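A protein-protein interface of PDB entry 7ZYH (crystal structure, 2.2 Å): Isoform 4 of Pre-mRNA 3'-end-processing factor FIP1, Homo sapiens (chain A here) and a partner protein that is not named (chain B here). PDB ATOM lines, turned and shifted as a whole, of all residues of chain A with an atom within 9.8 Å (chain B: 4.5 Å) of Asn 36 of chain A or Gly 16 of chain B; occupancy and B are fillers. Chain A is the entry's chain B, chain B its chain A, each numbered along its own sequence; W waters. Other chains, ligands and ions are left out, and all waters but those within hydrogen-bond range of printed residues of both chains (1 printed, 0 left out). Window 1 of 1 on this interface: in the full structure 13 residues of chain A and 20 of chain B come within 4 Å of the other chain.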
ATOM      1  N   ASP A  30     -26.514  13.955   5.206  1.00  0.00           N
ATOM      2  CA  ASP A  30     -25.310  14.472   5.852  1.00  0.00           C
ATOM      3  C   ASP A  30     -24.752  15.562   4.949  1.00  0.00           C
ATOM      4  O   ASP A  30     -24.352  15.281   3.814  1.00  0.00           O
ATOM      5  CB  ASP A  30     -24.271  13.369   6.055  1.00  0.00           C
ATOM      6  CG  ASP A  30     -24.724  12.317   7.042  1.00  0.00           C
ATOM      7  OD1 ASP A  30     -25.751  12.530   7.719  1.00  0.00           O
ATOM      8  OD2 ASP A  30     -24.043  11.276   7.146  1.00  0.00           O
ATOM      9  N   LEU A  31     -24.717  16.802   5.447  1.00  0.00           N
ATOM     10  CA  LEU A  31     -24.299  17.909   4.591  1.00  0.00           C
ATOM     11  C   LEU A  31     -22.959  17.625   3.927  1.00  0.00           C
ATOM     12  O   LEU A  31     -22.769  17.903   2.738  1.00  0.00           O
ATOM     13  CB  LEU A  31     -24.206  19.220   5.367  1.00  0.00           C
ATOM     14  CG  LEU A  31     -25.469  20.046   5.604  1.00  0.00           C
ATOM     15  CD1 LEU A  31     -25.168  21.172   6.613  1.00  0.00           C
ATOM     16  CD2 LEU A  31     -26.054  20.592   4.334  1.00  0.00           C
ATOM     17  N   SER A  32     -22.012  17.069   4.687  1.00  0.00           N
ATOM     18  CA  SER A  32     -20.657  16.870   4.183  1.00  0.00           C
ATOM     19  C   SER A  32     -20.638  16.132   2.856  1.00  0.00           C
ATOM     20  O   SER A  32     -19.682  16.271   2.092  1.00  0.00           O
ATOM     21  CB  SER A  32     -19.827  16.102   5.210  1.00  0.00           C
ATOM     22  OG  SER A  32     -20.341  14.798   5.404  1.00  0.00           O
ATOM     23  N   ASP A  33     -21.665  15.340   2.568  1.00  0.00           N
ATOM     24  CA  ASP A  33     -21.764  14.685   1.273  1.00  0.00           C
ATOM     25  C   ASP A  33     -21.981  15.686   0.145  1.00  0.00           C
ATOM     26  O   ASP A  33     -21.683  15.375  -1.013  1.00  0.00           O
ATOM     27  CB  ASP A  33     -22.905  13.667   1.300  1.00  0.00           C
ATOM     28  CG  ASP A  33     -22.492  12.340   1.902  1.00  0.00           C
ATOM     29  OD1 ASP A  33     -21.291  12.147   2.171  1.00  0.00           O
ATOM     30  OD2 ASP A  33     -23.377  11.496   2.136  1.00  0.00           O
ATOM     31  N   TYR A  34     -22.472  16.883   0.461  1.00  0.00           N
ATOM     32  CA  TYR A  34     -22.736  17.922  -0.528  1.00  0.00           C
ATOM     33  C   TYR A  34     -21.676  19.014  -0.522  1.00  0.00           C
ATOM     34  O   TYR A  34     -21.200  19.419  -1.584  1.00  0.00           O
ATOM     35  CB  TYR A  34     -24.112  18.545  -0.266  1.00  0.00           C
ATOM     36  CG  TYR A  34     -25.245  17.576  -0.494  1.00  0.00           C
ATOM     37  CD1 TYR A  34     -25.562  16.615   0.458  1.00  0.00           C
ATOM     38  CD2 TYR A  34     -25.998  17.620  -1.655  1.00  0.00           C
ATOM     39  CE1 TYR A  34     -26.586  15.719   0.249  1.00  0.00           C
ATOM     40  CE2 TYR A  34     -27.028  16.736  -1.865  1.00  0.00           C
ATOM     41  CZ  TYR A  34     -27.315  15.786  -0.911  1.00  0.00           C
ATOM     42  OH  TYR A  34     -28.339  14.896  -1.122  1.00  0.00           O
ATOM     43  N   PHE A  35     -21.298  19.494   0.656  1.00  0.00           N
ATOM     44  CA  PHE A  35     -20.379  20.609   0.798  1.00  0.00           C
ATOM     45  C   PHE A  35     -19.037  20.109   1.311  1.00  0.00           C
ATOM     46  O   PHE A  35     -18.988  19.307   2.245  1.00  0.00           O
ATOM     47  CB  PHE A  35     -20.953  21.649   1.756  1.00  0.00           C
ATOM     48  CG  PHE A  35     -22.251  22.237   1.298  1.00  0.00           C
ATOM     49  CD1 PHE A  35     -23.445  21.626   1.622  1.00  0.00           C
ATOM     50  CD2 PHE A  35     -22.280  23.407   0.553  1.00  0.00           C
ATOM     51  CE1 PHE A  35     -24.650  22.162   1.210  1.00  0.00           C
ATOM     52  CE2 PHE A  35     -23.482  23.951   0.138  1.00  0.00           C
ATOM     53  CZ  PHE A  35     -24.669  23.326   0.462  1.00  0.00           C
ATOM     54  N   ASN A  36     -17.958  20.592   0.702  1.00  0.00           N
ATOM     55  CA  ASN A  36     -16.607  20.273   1.128  1.00  0.00           C
ATOM     56  C   ASN A  36     -16.103  21.343   2.087  1.00  0.00           C
ATOM     57  O   ASN A  36     -16.720  22.386   2.286  1.00  0.00           O
ATOM     58  CB  ASN A  36     -15.681  20.159  -0.081  1.00  0.00           C
ATOM     59  CG  ASN A  36     -14.451  19.327   0.203  1.00  0.00           C
ATOM     60  OD1 ASN A  36     -14.157  19.007   1.351  1.00  0.00           O
ATOM     61  ND2 ASN A  36     -13.723  18.974  -0.848  1.00  0.00           N
ATOM     62  N   TYR A  37     -14.971  21.058   2.708  1.00  0.00           N
ATOM     63  CA  TYR A  37     -14.268  22.011   3.559  1.00  0.00           C
ATOM     64  C   TYR A  37     -15.096  22.489   4.738  1.00  0.00           C
ATOM     65  O   TYR A  37     -14.791  23.526   5.332  1.00  0.00           O
ATOM     66  CB  TYR A  37     -13.823  23.232   2.753  1.00  0.00           C
ATOM     67  CG  TYR A  37     -13.212  22.915   1.419  1.00  0.00           C
ATOM     68  CD1 TYR A  37     -12.008  22.252   1.338  1.00  0.00           C
ATOM     69  CD2 TYR A  37     -13.832  23.286   0.242  1.00  0.00           C
ATOM     70  CE1 TYR A  37     -11.432  21.964   0.121  1.00  0.00           C
ATOM     71  CE2 TYR A  37     -13.271  22.992  -0.976  1.00  0.00           C
ATOM     72  CZ  TYR A  37     -12.071  22.327  -1.031  1.00  0.00           C
ATOM     73  OH  TYR A  37     -11.495  22.030  -2.248  1.00  0.00           O
ATOM     74  N   GLY A  38     -16.139  21.766   5.104  1.00  0.00           N
ATOM     75  CA  GLY A  38     -16.936  22.209   6.223  1.00  0.00           C
ATOM     76  C   GLY A  38     -17.848  23.370   5.921  1.00  0.00           C
ATOM     77  O   GLY A  38     -18.285  24.062   6.846  1.00  0.00           O
ATOM     78  N   PHE A  39     -18.156  23.604   4.652  1.00  0.00           N
ATOM     79  CA  PHE A  39     -19.094  24.652   4.306  1.00  0.00           C
ATOM     80  C   PHE A  39     -20.474  24.329   4.847  1.00  0.00           C
ATOM     81  O   PHE A  39     -20.814  23.175   5.111  1.00  0.00           O
ATOM     82  CB  PHE A  39     -19.159  24.835   2.795  1.00  0.00           C
ATOM     83  CG  PHE A  39     -18.194  25.854   2.264  1.00  0.00           C
ATOM     84  CD1 PHE A  39     -18.414  27.198   2.500  1.00  0.00           C
ATOM     85  CD2 PHE A  39     -17.084  25.484   1.526  1.00  0.00           C
ATOM     86  CE1 PHE A  39     -17.547  28.155   2.013  1.00  0.00           C
ATOM     87  CE2 PHE A  39     -16.207  26.441   1.044  1.00  0.00           C
ATOM     88  CZ  PHE A  39     -16.440  27.777   1.295  1.00  0.00           C
ATOM     89  N   ASN A  40     -21.260  25.380   5.039  1.00  0.00           N
ATOM     90  CA  ASN A  40     -22.678  25.262   5.330  1.00  0.00           C
ATOM     91  C   ASN A  40     -23.494  25.766   4.153  1.00  0.00           C
ATOM     92  O   ASN A  40     -22.972  26.353   3.208  1.00  0.00           O
ATOM     93  CB  ASN A  40     -23.050  26.088   6.568  1.00  0.00           C
ATOM     94  CG  ASN A  40     -23.129  25.263   7.819  1.00  0.00           C
ATOM     95  OD1 ASN A  40     -24.024  24.437   7.965  1.00  0.00           O
ATOM     96  ND2 ASN A  40     -22.210  25.497   8.746  1.00  0.00           N
ATOM     97  N   GLU A  41     -24.799  25.511   4.212  1.00  0.00           N
ATOM     98  CA  GLU A  41     -25.690  26.113   3.232  1.00  0.00           C
ATOM     99  C   GLU A  41     -25.499  27.624   3.235  1.00  0.00           C
ATOM    100  O   GLU A  41     -25.344  28.253   2.186  1.00  0.00           O
ATOM    101  CB  GLU A  41     -27.133  25.747   3.554  1.00  0.00           C
ATOM    102  CG  GLU A  41     -28.141  26.210   2.512  1.00  0.00           C
ATOM    103  CD  GLU A  41     -29.582  25.994   2.953  1.00  0.00           C
ATOM    104  OE1 GLU A  41     -29.810  25.208   3.900  1.00  0.00           O
ATOM    105  OE2 GLU A  41     -30.486  26.614   2.348  1.00  0.00           O
ATOM    106  N   THR A  43     -22.938  29.314   4.751  1.00  0.00           N
ATOM    107  CA  THR A  43     -21.561  29.719   4.537  1.00  0.00           C
ATOM    108  C   THR A  43     -21.184  29.601   3.065  1.00  0.00           C
ATOM    109  O   THR A  43     -20.403  30.400   2.548  1.00  0.00           O
ATOM    110  CB  THR A  43     -20.608  28.888   5.403  1.00  0.00           C
ATOM    111  OG1 THR A  43     -21.143  28.758   6.724  1.00  0.00           O
ATOM    112  CG2 THR A  43     -19.247  29.569   5.480  1.00  0.00           C
ATOM    113  N   TRP A  44     -21.687  28.571   2.380  1.00  0.00           N
ATOM    114  CA  TRP A  44     -21.436  28.459   0.948  1.00  0.00           C
ATOM    115  C   TRP A  44     -22.077  29.599   0.177  1.00  0.00           C
ATOM    116  O   TRP A  44     -21.441  30.211  -0.683  1.00  0.00           O
ATOM    117  CB  TRP A  44     -21.957  27.123   0.424  1.00  0.00           C
ATOM    118  CG  TRP A  44     -21.899  27.007  -1.083  1.00  0.00           C
ATOM    119  CD1 TRP A  44     -22.965  27.022  -1.941  1.00  0.00           C
ATOM    120  CD2 TRP A  44     -20.728  26.890  -1.906  1.00  0.00           C
ATOM    121  NE1 TRP A  44     -22.532  26.909  -3.240  1.00  0.00           N
ATOM    122  CE2 TRP A  44     -21.164  26.829  -3.246  1.00  0.00           C
ATOM    123  CE3 TRP A  44     -19.359  26.828  -1.642  1.00  0.00           C
ATOM    124  CZ2 TRP A  44     -20.280  26.706  -4.313  1.00  0.00           C
ATOM    125  CZ3 TRP A  44     -18.481  26.705  -2.707  1.00  0.00           C
ATOM    126  CH2 TRP A  44     -18.945  26.645  -4.022  1.00  0.00           C
ATOM    127  N   LYS A  45     -23.342  29.897   0.463  1.00  0.00           N
ATOM    128  CA  LYS A  45     -23.982  31.036  -0.188  1.00  0.00           C
ATOM    129  C   LYS A  45     -23.197  32.315   0.077  1.00  0.00           C
ATOM    130  O   LYS A  45     -22.954  33.117  -0.834  1.00  0.00           O
ATOM    131  CB  LYS A  45     -25.439  31.161   0.263  1.00  0.00           C
ATOM    132  CG  LYS A  45     -26.338  30.080  -0.353  1.00  0.00           C
ATOM    133  CD  LYS A  45     -27.787  30.533  -0.480  1.00  0.00           C
ATOM    134  CE  LYS A  45     -28.418  29.996  -1.771  1.00  0.00           C
ATOM    135  NZ  LYS A  45     -28.993  31.087  -2.629  1.00  0.00           N
ATOM    136  N   TYR A  47     -20.121  32.526   0.646  1.00  0.00           N
ATOM    137  CA  TYR A  47     -18.880  32.431  -0.112  1.00  0.00           C
ATOM    138  C   TYR A  47     -19.118  32.800  -1.570  1.00  0.00           C
ATOM    139  O   TYR A  47     -18.280  33.457  -2.194  1.00  0.00           O
ATOM    140  CB  TYR A  47     -18.305  31.020   0.027  1.00  0.00           C
ATOM    141  CG  TYR A  47     -17.084  30.716  -0.816  1.00  0.00           C
ATOM    142  CD1 TYR A  47     -15.879  31.370  -0.590  1.00  0.00           C
ATOM    143  CD2 TYR A  47     -17.126  29.757  -1.816  1.00  0.00           C
ATOM    144  CE1 TYR A  47     -14.760  31.086  -1.342  1.00  0.00           C
ATOM    145  CE2 TYR A  47     -16.010  29.468  -2.578  1.00  0.00           C
ATOM    146  CZ  TYR A  47     -14.829  30.118  -2.322  1.00  0.00           C
ATOM    147  OH  TYR A  47     -13.718  29.844  -3.081  1.00  0.00           O
ATOM    148  N   CYS A  48     -20.268  32.407  -2.119  1.00  0.00           N
ATOM    149  CA  CYS A  48     -20.588  32.777  -3.489  1.00  0.00           C
ATOM    150  C   CYS A  48     -20.852  34.272  -3.613  1.00  0.00           C
ATOM    151  O   CYS A  48     -20.393  34.899  -4.568  1.00  0.00           O
ATOM    152  CB  CYS A  48     -21.792  31.976  -3.979  1.00  0.00           C
ATOM    153  SG  CYS A  48     -21.531  30.215  -4.090  1.00  0.00           S
ATOM    154  N   GLN A  51     -17.550  35.957  -3.686  1.00  0.00           N
ATOM    155  CA  GLN A  51     -16.988  35.787  -5.019  1.00  0.00           C
ATOM    156  C   GLN A  51     -17.597  36.794  -5.979  1.00  0.00           C
ATOM    157  O   GLN A  51     -16.888  37.477  -6.722  1.00  0.00           O
ATOM    158  CB  GLN A  51     -17.242  34.380  -5.532  1.00  0.00           C
ATOM    159  CG  GLN A  51     -16.545  33.335  -4.727  1.00  0.00           C
ATOM    160  CD  GLN A  51     -15.065  33.195  -5.069  1.00  0.00           C
ATOM    161  OE1 GLN A  51     -14.562  33.908  -5.924  1.00  0.00           O
ATOM    162  NE2 GLN A  51     -14.367  32.268  -4.395  1.00  0.00           N
ATOM    163  N   TRP B  12     -16.718  19.094  -8.768  1.00  0.00           N
ATOM    164  CA  TRP B  12     -17.633  20.068  -8.177  1.00  0.00           C
ATOM    165  C   TRP B  12     -17.463  20.118  -6.661  1.00  0.00           C
ATOM    166  O   TRP B  12     -17.507  21.197  -6.060  1.00  0.00           O
ATOM    167  CB  TRP B  12     -19.082  19.730  -8.547  1.00  0.00           C
ATOM    168  CG  TRP B  12     -19.395  19.836 -10.011  1.00  0.00           C
ATOM    169  CD1 TRP B  12     -19.339  18.841 -10.934  1.00  0.00           C
ATOM    170  CD2 TRP B  12     -19.850  21.004 -10.705  1.00  0.00           C
ATOM    171  NE1 TRP B  12     -19.707  19.320 -12.167  1.00  0.00           N
ATOM    172  CE2 TRP B  12     -20.029  20.646 -12.053  1.00  0.00           C
ATOM    173  CE3 TRP B  12     -20.116  22.319 -10.317  1.00  0.00           C
ATOM    174  CZ2 TRP B  12     -20.463  21.557 -13.019  1.00  0.00           C
ATOM    175  CZ3 TRP B  12     -20.547  23.223 -11.279  1.00  0.00           C
ATOM    176  CH2 TRP B  12     -20.718  22.836 -12.612  1.00  0.00           C
ATOM    177  N   TYR B  13     -17.259  18.961  -6.034  1.00  0.00           N
ATOM    178  CA  TYR B  13     -17.005  18.920  -4.602  1.00  0.00           C
ATOM    179  C   TYR B  13     -15.679  19.591  -4.286  1.00  0.00           C
ATOM    180  O   TYR B  13     -15.539  20.248  -3.250  1.00  0.00           O
ATOM    181  CB  TYR B  13     -17.027  17.468  -4.124  1.00  0.00           C
ATOM    182  CG  TYR B  13     -17.130  17.316  -2.629  1.00  0.00           C
ATOM    183  CD1 TYR B  13     -18.309  17.610  -1.964  1.00  0.00           C
ATOM    184  CD2 TYR B  13     -16.051  16.862  -1.883  1.00  0.00           C
ATOM    185  CE1 TYR B  13     -18.407  17.474  -0.595  1.00  0.00           C
ATOM    186  CE2 TYR B  13     -16.142  16.716  -0.514  1.00  0.00           C
ATOM    187  CZ  TYR B  13     -17.322  17.024   0.122  1.00  0.00           C
ATOM    188  OH  TYR B  13     -17.418  16.883   1.482  1.00  0.00           O
ATOM    189  N   ASP B  14     -14.693  19.426  -5.170  1.00  0.00           N
ATOM    190  CA  ASP B  14     -13.398  20.060  -4.962  1.00  0.00           C
ATOM    191  C   ASP B  14     -13.518  21.572  -5.016  1.00  0.00           C
ATOM    192  O   ASP B  14     -12.755  22.282  -4.355  1.00  0.00           O
ATOM    193  CB  ASP B  14     -12.413  19.587  -6.030  1.00  0.00           C
ATOM    194  CG  ASP B  14     -12.067  18.122  -5.898  1.00  0.00           C
ATOM    195  OD1 ASP B  14     -12.717  17.424  -5.091  1.00  0.00           O
ATOM    196  OD2 ASP B  14     -11.162  17.660  -6.623  1.00  0.00           O
ATOM    197  N   ARG B  15     -14.460  22.083  -5.804  1.00  0.00           N
ATOM    198  CA  ARG B  15     -14.782  23.499  -5.742  1.00  0.00           C
ATOM    199  C   ARG B  15     -15.453  23.863  -4.427  1.00  0.00           C
ATOM    200  O   ARG B  15     -15.309  24.996  -3.955  1.00  0.00           O
ATOM    201  CB  ARG B  15     -15.726  23.869  -6.876  1.00  0.00           C
ATOM    202  CG  ARG B  15     -16.081  25.345  -6.962  1.00  0.00           C
ATOM    203  CD  ARG B  15     -17.258  25.515  -7.909  1.00  0.00           C
ATOM    204  NE  ARG B  15     -17.530  26.901  -8.256  1.00  0.00           N
ATOM    205  CZ  ARG B  15     -18.718  27.357  -8.623  1.00  0.00           C
ATOM    206  NH1 ARG B  15     -19.801  26.603  -8.552  1.00  0.00           N
ATOM    207  NH2 ARG B  15     -18.820  28.598  -9.086  1.00  0.00           N
ATOM    208  N   GLY B  16     -16.207  22.932  -3.839  1.00  0.00           N
ATOM    209  CA  GLY B  16     -16.800  23.158  -2.536  1.00  0.00           C
ATOM    210  C   GLY B  16     -18.233  22.704  -2.354  1.00  0.00           C
ATOM    211  O   GLY B  16     -18.699  22.579  -1.220  1.00  0.00           O
ATOM    212  N   PHE B  17     -18.944  22.453  -3.447  1.00  0.00           N
ATOM    213  CA  PHE B  17     -20.353  22.082  -3.371  1.00  0.00           C
ATOM    214  C   PHE B  17     -20.754  21.246  -4.573  1.00  0.00           C
ATOM    215  O   PHE B  17     -20.446  21.611  -5.708  1.00  0.00           O
ATOM    216  CB  PHE B  17     -21.268  23.311  -3.287  1.00  0.00           C
ATOM    217  CG  PHE B  17     -22.716  23.001  -3.571  1.00  0.00           C
ATOM    218  CD1 PHE B  17     -23.501  22.337  -2.648  1.00  0.00           C
ATOM    219  CD2 PHE B  17     -23.286  23.368  -4.777  1.00  0.00           C
ATOM    220  CE1 PHE B  17     -24.822  22.047  -2.925  1.00  0.00           C
ATOM    221  CE2 PHE B  17     -24.606  23.087  -5.053  1.00  0.00           C
ATOM    222  CZ  PHE B  17     -25.374  22.425  -4.126  1.00  0.00           C
ATOM    223  N   THR B  29     -14.070  13.329  -1.798  1.00  0.00           N
ATOM    224  CA  THR B  29     -13.023  13.381  -0.789  1.00  0.00           C
ATOM    225  C   THR B  29     -13.129  14.660   0.039  1.00  0.00           C
ATOM    226  O   THR B  29     -13.052  15.769  -0.496  1.00  0.00           O
ATOM    227  CB  THR B  29     -11.649  13.315  -1.450  1.00  0.00           C
ATOM    228  OG1 THR B  29     -11.566  12.182  -2.319  1.00  0.00           O
ATOM    229  CG2 THR B  29     -10.562  13.215  -0.392  1.00  0.00           C
ATOM    230  N   ARG B  30     -13.312  14.500   1.346  1.00  0.00           N
ATOM    231  CA  ARG B  30     -13.373  15.636   2.251  1.00  0.00           C
ATOM    232  C   ARG B  30     -11.986  16.242   2.374  1.00  0.00           C
ATOM    233  O   ARG B  30     -11.007  15.540   2.635  1.00  0.00           O
ATOM    234  CB  ARG B  30     -13.906  15.175   3.603  1.00  0.00           C
ATOM    235  CG  ARG B  30     -15.429  15.030   3.645  1.00  0.00           C
ATOM    236  CD  ARG B  30     -15.898  14.505   5.013  1.00  0.00           C
ATOM    237  NE  ARG B  30     -15.538  13.100   5.191  1.00  0.00           N
ATOM    238  CZ  ARG B  30     -15.227  12.528   6.346  1.00  0.00           C
ATOM    239  NH1 ARG B  30     -15.149  13.225   7.466  1.00  0.00           N
ATOM    240  NH2 ARG B  30     -15.001  11.216   6.378  1.00  0.00           N
ATOM    241  N   ARG B  31     -11.914  17.557   2.215  1.00  0.00           N
ATOM    242  CA  ARG B  31     -10.659  18.281   2.167  1.00  0.00           C
ATOM    243  C   ARG B  31     -10.750  19.434   3.162  1.00  0.00           C
ATOM    244  O   ARG B  31     -11.820  19.741   3.693  1.00  0.00           O
ATOM    245  CB  ARG B  31     -10.403  18.843   0.758  1.00  0.00           C
ATOM    246  CG  ARG B  31     -10.137  17.860  -0.396  1.00  0.00           C
ATOM    247  CD  ARG B  31      -8.736  17.252  -0.538  1.00  0.00           C
ATOM    248  NE  ARG B  31      -8.682  16.504  -1.798  1.00  0.00           N
ATOM    249  CZ  ARG B  31      -8.277  15.248  -1.933  1.00  0.00           C
ATOM    250  NH1 ARG B  31      -7.874  14.539  -0.895  1.00  0.00           N
ATOM    251  NH2 ARG B  31      -8.282  14.689  -3.141  1.00  0.00           N
HETATM  252  O   HOH W   1     -12.137  17.753  -2.603  1.00  0.00           O
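OH of Tyr 13 of chain B is in hydrogen-bond range of O of Ser 32 of chain A, at 2.4 Å.
The side-chain hydroxyl of Tyr 13 of chain B is in hydrogen-bond range of the backbone carbonyl oxygen of Phe 35 of chain A (3.0 Å).
The side-chain amide nitrogen (ND2) of Asn 36 of chain A sits close to the backbone carbonyl oxygen (O) of Tyr 13 of chain B (3.3 Å).
O of Asp 14 of chain B sits at hydrogen-bond distance from OH of Tyr 37 of chain A, at 2.5 Å.
N of Asn 36 of chain A is in hydrogen-bond range of O of Gly 16 of chain B, at 2.9 Å.
The backbone carbonyl oxygen (O) of Thr 29 of chain B sits at hydrogen-bond distance from the side-chain amide nitrogen (ND2) of Asn 36 of chain A.
The backbone NH of Arg 31 of chain B sits at hydrogen-bond distance from the side-chain amide oxygen of Asn 36 of chain A (2.8 Å).
Asn 36 of chain A touches just these residues of chain B: Tyr 13 (3.2 Å), Gly 16 (2.9 Å), Thr 29 (3.3 Å), Arg 30 (3.6 Å) and Arg 31 (2.8 Å).
Gly 16 of chain B touches four residues of chain A.
Of the printed residues of chain B, Tyr 34 of chain A touches Tyr 13 (3.4 Å) and Phe 17 (3.3 Å).
Of the printed residues of chain B, Tyr 37 of chain A touches Asp 14 (2.5 Å), Gly 16 (3.9 Å) and Arg 31 (3.3 Å).
The nearest residue of chain B that does not touch Asn 36 of chain A is Asp 14 of chain B (4.3 Å).
The nearest printed residue of chain A that does not touch Phe 17 of chain B is Asn 36 of chain A (4.7 Å).
Water W1 lies within hydrogen-bond range of the side-chain carboxylate (OD1) of Asp 14 of chain B (2.6 Å), the side-chain amide nitrogen (ND2) of Asn 36 of chain A (2.7 Å) and the backbone carbonyl oxygen (O) of Thr 29 of chain B (3.0 Å).
Among the printed residues, merely in contact across the chains: Phe 35 of chain A with Phe 17 of chain B (3.2 Å), Phe 35 of chain A with Gly 16 of chain B (3.3 Å), Tyr 34 of chain A with Phe 17 of chain B (3.3 Å), Tyr 37 of chain A with Arg 31 of chain B (3.3 Å), Tyr 34 of chain A with Tyr 13 of chain B (3.4 Å), Trp 44 of chain A with Phe 17 of chain B (3.5 Å), Asn 36 of chain A with Arg 30 of chain B (3.6 Å), Trp 44 of chain A with Arg 15 of chain B (3.8 Å), Tyr 37 of chain A with Gly 16 of chain B (3.9 Å), Asp 33 of chain A with Tyr 13 of chain B (3.9 Å) and Trp 44 of chain A with Gly 16 of chain B (3.9 Å).
Among the printed residues, no Asp or Glu carboxylate lies within 4 Å of a Lys or Arg side-chain nitrogen of the other chain.
N of Phe 17 of chain B is in hydrogen-bond range of O of Trp 12 of chain B, at 3.2 Å.
SG of Cys 48 of chain A lies within hydrogen-bond range of O of Trp 44 of chain A, at 3.4 Å.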
